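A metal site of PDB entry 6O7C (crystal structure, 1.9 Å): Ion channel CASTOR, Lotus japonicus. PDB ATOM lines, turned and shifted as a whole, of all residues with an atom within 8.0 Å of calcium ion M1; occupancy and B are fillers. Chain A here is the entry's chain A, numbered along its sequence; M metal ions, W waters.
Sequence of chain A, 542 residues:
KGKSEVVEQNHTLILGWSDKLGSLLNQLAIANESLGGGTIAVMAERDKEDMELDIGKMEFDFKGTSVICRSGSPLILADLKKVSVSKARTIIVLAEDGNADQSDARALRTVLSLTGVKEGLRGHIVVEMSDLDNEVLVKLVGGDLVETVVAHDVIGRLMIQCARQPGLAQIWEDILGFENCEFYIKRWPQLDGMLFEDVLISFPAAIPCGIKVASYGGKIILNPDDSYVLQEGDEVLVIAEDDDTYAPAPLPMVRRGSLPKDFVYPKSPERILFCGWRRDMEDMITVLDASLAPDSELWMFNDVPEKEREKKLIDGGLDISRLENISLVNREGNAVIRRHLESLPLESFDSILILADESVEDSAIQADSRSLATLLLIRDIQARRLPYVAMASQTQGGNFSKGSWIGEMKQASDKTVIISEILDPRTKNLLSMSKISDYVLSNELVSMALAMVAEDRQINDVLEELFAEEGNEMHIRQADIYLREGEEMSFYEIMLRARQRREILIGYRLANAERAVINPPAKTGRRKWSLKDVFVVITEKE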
ATOM      1  N   GLN A  27      26.544   2.975 -10.738  1.00  0.00           N
ATOM      2  CA  GLN A  27      25.151   2.959 -10.268  1.00  0.00           C
ATOM      3  C   GLN A  27      24.506   1.600 -10.475  1.00  0.00           C
ATOM      4  O   GLN A  27      23.773   1.103  -9.590  1.00  0.00           O
ATOM      5  CB  GLN A  27      24.323   4.038 -10.994  1.00  0.00           C
ATOM      6  CG  GLN A  27      24.712   5.458 -10.585  1.00  0.00           C
ATOM      7  CD  GLN A  27      24.485   5.704  -9.085  1.00  0.00           C
ATOM      8  OE1 GLN A  27      23.481   5.302  -8.567  1.00  0.00           O
ATOM      9  NE2 GLN A  27      25.425   6.332  -8.419  1.00  0.00           N
ATOM     10  N   ILE A  30      25.804  -0.802  -7.960  1.00  0.00           N
ATOM     11  CA  ILE A  30      25.123  -0.593  -6.661  1.00  0.00           C
ATOM     12  C   ILE A  30      23.729  -1.227  -6.683  1.00  0.00           C
ATOM     13  O   ILE A  30      23.338  -1.968  -5.762  1.00  0.00           O
ATOM     14  CB  ILE A  30      25.076   0.905  -6.316  1.00  0.00           C
ATOM     15  CG1 ILE A  30      26.521   1.478  -6.184  1.00  0.00           C
ATOM     16  CG2 ILE A  30      24.294   1.087  -4.982  1.00  0.00           C
ATOM     17  CD1 ILE A  30      26.489   3.057  -6.247  1.00  0.00           C
ATOM     18  N   ALA A  31      22.976  -0.990  -7.769  1.00  0.00           N
ATOM     19  CA  ALA A  31      21.642  -1.547  -7.891  1.00  0.00           C
ATOM     20  C   ALA A  31      21.708  -3.085  -7.880  1.00  0.00           C
ATOM     21  O   ALA A  31      20.833  -3.755  -7.317  1.00  0.00           O
ATOM     22  CB  ALA A  31      20.936  -1.053  -9.172  1.00  0.00           C
ATOM     23  N   ASP A 174      21.027  12.574  -2.821  1.00  0.00           N
ATOM     24  CA  ASP A 174      20.776  11.359  -2.040  1.00  0.00           C
ATOM     25  C   ASP A 174      19.751  10.453  -2.699  1.00  0.00           C
ATOM     26  O   ASP A 174      19.943   9.225  -2.735  1.00  0.00           O
ATOM     27  CB  ASP A 174      20.270  11.692  -0.626  1.00  0.00           C
ATOM     28  CG  ASP A 174      21.387  12.089   0.350  1.00  0.00           C
ATOM     29  OD1 ASP A 174      22.605  11.914   0.072  1.00  0.00           O
ATOM     30  OD2 ASP A 174      20.984  12.503   1.481  1.00  0.00           O
ATOM     31  N   ILE A 175      18.638  11.028  -3.178  1.00  0.00           N
ATOM     32  CA  ILE A 175      17.532  10.219  -3.681  1.00  0.00           C
ATOM     33  C   ILE A 175      17.843   9.645  -5.045  1.00  0.00           C
ATOM     34  O   ILE A 175      17.427   8.513  -5.349  1.00  0.00           O
ATOM     35  CB  ILE A 175      16.235  11.057  -3.677  1.00  0.00           C
ATOM     36  CG1 ILE A 175      15.845  11.216  -2.219  1.00  0.00           C
ATOM     37  CG2 ILE A 175      15.142  10.333  -4.397  1.00  0.00           C
ATOM     38  CD1 ILE A 175      14.554  12.026  -2.040  1.00  0.00           C
ATOM     39  N   LEU A 176      18.477  10.407  -5.929  1.00  0.00           N
ATOM     40  CA  LEU A 176      18.812   9.871  -7.245  1.00  0.00           C
ATOM     41  C   LEU A 176      19.865   8.756  -7.155  1.00  0.00           C
ATOM     42  O   LEU A 176      20.652   8.677  -6.215  1.00  0.00           O
ATOM     43  CB  LEU A 176      19.376  11.031  -8.127  1.00  0.00           C
ATOM     44  CG  LEU A 176      18.338  12.076  -8.533  1.00  0.00           C
ATOM     45  CD1 LEU A 176      19.019  13.243  -9.330  1.00  0.00           C
ATOM     46  CD2 LEU A 176      17.236  11.485  -9.294  1.00  0.00           C
ATOM     47  N   GLY A 177      19.858   7.877  -8.155  1.00  0.00           N
ATOM     48  CA  GLY A 177      20.875   6.851  -8.100  1.00  0.00           C
ATOM     49  C   GLY A 177      20.607   5.809  -6.964  1.00  0.00           C
ATOM     50  O   GLY A 177      19.533   5.801  -6.325  1.00  0.00           O
ATOM     51  N   PHE A 178      21.582   4.982  -6.693  1.00  0.00           N
ATOM     52  CA  PHE A 178      21.286   3.834  -5.842  1.00  0.00           C
ATOM     53  C   PHE A 178      22.052   3.810  -4.527  1.00  0.00           C
ATOM     54  O   PHE A 178      21.692   3.012  -3.642  1.00  0.00           O
ATOM     55  CB  PHE A 178      21.478   2.510  -6.633  1.00  0.00           C
ATOM     56  CG  PHE A 178      20.374   2.275  -7.590  1.00  0.00           C
ATOM     57  CD1 PHE A 178      19.191   1.718  -7.167  1.00  0.00           C
ATOM     58  CD2 PHE A 178      20.470   2.717  -8.954  1.00  0.00           C
ATOM     59  CE1 PHE A 178      18.144   1.521  -8.021  1.00  0.00           C
ATOM     60  CE2 PHE A 178      19.369   2.541  -9.810  1.00  0.00           C
ATOM     61  CZ  PHE A 178      18.225   1.959  -9.369  1.00  0.00           C
ATOM     62  N   GLU A 179      23.004   4.725  -4.277  1.00  0.00           N
ATOM     63  CA  GLU A 179      23.472   4.888  -2.908  1.00  0.00           C
ATOM     64  C   GLU A 179      22.313   5.401  -2.050  1.00  0.00           C
ATOM     65  O   GLU A 179      21.452   6.103  -2.543  1.00  0.00           O
ATOM     66  CB  GLU A 179      24.602   5.922  -2.822  1.00  0.00           C
ATOM     67  CG  GLU A 179      25.614   5.941  -3.905  1.00  0.00           C
ATOM     68  CD  GLU A 179      25.223   6.782  -5.230  1.00  0.00           C
ATOM     69  OE1 GLU A 179      24.014   7.036  -5.592  1.00  0.00           O
ATOM     70  OE2 GLU A 179      26.220   7.287  -5.847  1.00  0.00           O
ATOM     71  N   ASN A 180      22.308   5.098  -0.757  1.00  0.00           N
ATOM     72  CA  ASN A 180      21.230   5.602   0.190  1.00  0.00           C
ATOM     73  C   ASN A 180      19.882   5.046  -0.281  1.00  0.00           C
ATOM     74  O   ASN A 180      19.786   3.879  -0.640  1.00  0.00           O
ATOM     75  CB  ASN A 180      21.244   7.121   0.257  1.00  0.00           C
ATOM     76  CG  ASN A 180      22.704   7.716   0.422  1.00  0.00           C
ATOM     77  OD1 ASN A 180      23.228   8.356  -0.520  1.00  0.00           O
ATOM     78  ND2 ASN A 180      23.296   7.511   1.531  1.00  0.00           N
ATOM     79  N   CYS A 181      18.801   5.854  -0.210  1.00  0.00           N
ATOM     80  CA  CYS A 181      17.424   5.432  -0.494  1.00  0.00           C
ATOM     81  C   CYS A 181      16.918   5.971  -1.829  1.00  0.00           C
ATOM     82  O   CYS A 181      17.327   7.059  -2.278  1.00  0.00           O
ATOM     83  CB  CYS A 181      16.517   5.910   0.680  1.00  0.00           C
ATOM     84  SG  CYS A 181      16.877   5.016   2.271  1.00  0.00           S
ATOM     85  N   GLU A 182      16.016   5.229  -2.477  1.00  0.00           N
ATOM     86  CA  GLU A 182      15.438   5.632  -3.779  1.00  0.00           C
ATOM     87  C   GLU A 182      14.031   5.029  -3.934  1.00  0.00           C
ATOM     88  O   GLU A 182      13.488   4.408  -3.025  1.00  0.00           O
ATOM     89  CB  GLU A 182      16.379   5.245  -4.953  1.00  0.00           C
ATOM     90  CG  GLU A 182      16.716   3.701  -4.948  1.00  0.00           C
ATOM     91  CD  GLU A 182      17.941   3.347  -4.021  1.00  0.00           C
ATOM     92  OE1 GLU A 182      18.673   4.195  -3.419  1.00  0.00           O
ATOM     93  OE2 GLU A 182      18.041   2.130  -3.770  1.00  0.00           O
ATOM     94  N   PHE A 183      13.430   5.206  -5.130  1.00  0.00           N
ATOM     95  CA  PHE A 183      12.075   4.751  -5.326  1.00  0.00           C
ATOM     96  C   PHE A 183      12.016   3.272  -5.754  1.00  0.00           C
ATOM     97  O   PHE A 183      12.818   2.821  -6.566  1.00  0.00           O
ATOM     98  CB  PHE A 183      11.400   5.601  -6.429  1.00  0.00           C
ATOM     99  CG  PHE A 183      11.292   7.043  -6.064  1.00  0.00           C
ATOM    100  CD1 PHE A 183      10.336   7.444  -5.135  1.00  0.00           C
ATOM    101  CD2 PHE A 183      12.126   8.002  -6.625  1.00  0.00           C
ATOM    102  CE1 PHE A 183      10.192   8.778  -4.733  1.00  0.00           C
ATOM    103  CE2 PHE A 183      12.056   9.353  -6.248  1.00  0.00           C
ATOM    104  CZ  PHE A 183      11.056   9.763  -5.277  1.00  0.00           C
ATOM    105  N   TYR A 184      11.027   2.538  -5.230  1.00  0.00           N
ATOM    106  CA  TYR A 184      10.759   1.179  -5.644  1.00  0.00           C
ATOM    107  C   TYR A 184       9.264   1.022  -5.794  1.00  0.00           C
ATOM    108  O   TYR A 184       8.496   1.601  -5.034  1.00  0.00           O
ATOM    109  CB  TYR A 184      11.287   0.116  -4.672  1.00  0.00           C
ATOM    110  CG  TYR A 184      12.821   0.098  -4.723  1.00  0.00           C
ATOM    111  CD1 TYR A 184      13.502  -0.546  -5.762  1.00  0.00           C
ATOM    112  CD2 TYR A 184      13.551   0.782  -3.801  1.00  0.00           C
ATOM    113  CE1 TYR A 184      14.883  -0.513  -5.839  1.00  0.00           C
ATOM    114  CE2 TYR A 184      14.935   0.777  -3.848  1.00  0.00           C
ATOM    115  CZ  TYR A 184      15.577   0.149  -4.881  1.00  0.00           C
ATOM    116  OH  TYR A 184      16.984   0.204  -4.960  1.00  0.00           O
ATOM    117  N   ALA A 240      12.849   3.562  -0.306  1.00  0.00           N
ATOM    118  CA  ALA A 240      13.440   2.560   0.591  1.00  0.00           C
ATOM    119  C   ALA A 240      14.905   2.387   0.279  1.00  0.00           C
ATOM    120  O   ALA A 240      15.411   2.857  -0.732  1.00  0.00           O
ATOM    121  CB  ALA A 240      12.710   1.209   0.468  1.00  0.00           C
ATOM    122  N   GLU A 241      15.609   1.673   1.168  1.00  0.00           N
ATOM    123  CA  GLU A 241      17.073   1.623   0.952  1.00  0.00           C
ATOM    124  C   GLU A 241      17.428   0.741  -0.238  1.00  0.00           C
ATOM    125  O   GLU A 241      18.452   0.948  -0.872  1.00  0.00           O
ATOM    126  CB  GLU A 241      17.806   1.107   2.221  1.00  0.00           C
ATOM    127  CG  GLU A 241      19.352   1.110   2.130  1.00  0.00           C
ATOM    128  CD  GLU A 241      20.114   0.369   3.277  1.00  0.00           C
ATOM    129  OE1 GLU A 241      19.482  -0.105   4.248  1.00  0.00           O
ATOM    130  OE2 GLU A 241      21.366   0.198   3.159  1.00  0.00           O
ATOM    131  N   ASP A 242      16.682  -0.352  -0.508  1.00  0.00           N
ATOM    132  CA  ASP A 242      17.030  -1.217  -1.637  1.00  0.00           C
ATOM    133  C   ASP A 242      15.732  -1.952  -1.969  1.00  0.00           C
ATOM    134  O   ASP A 242      14.725  -1.781  -1.266  1.00  0.00           O
ATOM    135  CB  ASP A 242      18.161  -2.191  -1.242  1.00  0.00           C
ATOM    136  CG  ASP A 242      19.031  -2.622  -2.439  1.00  0.00           C
ATOM    137  OD1 ASP A 242      18.526  -2.570  -3.565  1.00  0.00           O
ATOM    138  OD2 ASP A 242      20.236  -2.909  -2.217  1.00  0.00           O
ATOM    139  N   ASP A 243      15.747  -2.756  -3.047  1.00  0.00           N
ATOM    140  CA  ASP A 243      14.491  -3.340  -3.449  1.00  0.00           C
ATOM    141  C   ASP A 243      13.997  -4.387  -2.444  1.00  0.00           C
ATOM    142  O   ASP A 243      12.799  -4.754  -2.491  1.00  0.00           O
ATOM    143  CB  ASP A 243      14.553  -4.017  -4.859  1.00  0.00           C
ATOM    144  CG  ASP A 243      15.705  -4.999  -4.979  1.00  0.00           C
ATOM    145  OD1 ASP A 243      16.881  -4.566  -5.018  1.00  0.00           O
ATOM    146  OD2 ASP A 243      15.488  -6.233  -4.746  1.00  0.00           O
ATOM    147  N   THR A 245      14.700  -4.500   1.159  1.00  0.00           N
ATOM    148  CA  THR A 245      14.971  -4.176   2.560  1.00  0.00           C
ATOM    149  C   THR A 245      13.709  -3.841   3.321  1.00  0.00           C
ATOM    150  O   THR A 245      13.776  -3.597   4.541  1.00  0.00           O
ATOM    151  CB  THR A 245      15.933  -2.981   2.661  1.00  0.00           C
ATOM    152  OG1 THR A 245      15.370  -1.913   1.910  1.00  0.00           O
ATOM    153  CG2 THR A 245      17.320  -3.339   2.129  1.00  0.00           C
HETATM  154 CA    CA M   1      19.947   2.235  -2.289  1.00  0.00          CA
HETATM  155 CA    CA M   2      19.105  -3.945  -5.585  1.00  0.00          CA
HETATM  156  O   HOH W   1      21.709   1.336  -0.791  1.00  0.00           O
HETATM  157  O   HOH W   2      20.352   0.158  -3.466  1.00  0.00           O
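N of Phe 178 lies within hydrogen-bond range of OE1 of Gln 27 (2.7 Å).
N of Glu 241 lies close to SG of Cys 181 (3.7 Å).
NE2 of Gln 27 sits at hydrogen-bond distance from OE2 of Glu 179 (2.9 Å).
OE2 of Glu 182 lies close to OH of Tyr 184 (2.5 Å).
The backbone carbonyl oxygen of Glu 182 lies within hydrogen-bond range of the backbone NH of Ala 240 (2.9 Å).
Merely in contact with calcium ion M1: Glu 179.
The nearest printed residue that does not touch calcium ion M1 is Cys 181 (4.3 Å).
Calcium ion M1 is bound by the backbone carbonyl oxygen (O) of Asn 180 (2.3 Å), the backbone carbonyl oxygen (O) of Phe 178 (2.3 Å), the side-chain carboxylate (OE2) of Glu 182 (2.4 Å), water W2 (2.4 Å), the backbone carbonyl oxygen (O) of Glu 241 (2.4 Å), water W1 (2.5 Å) and the side-chain carboxylate (OE1) of Glu 182 (2.6 Å).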
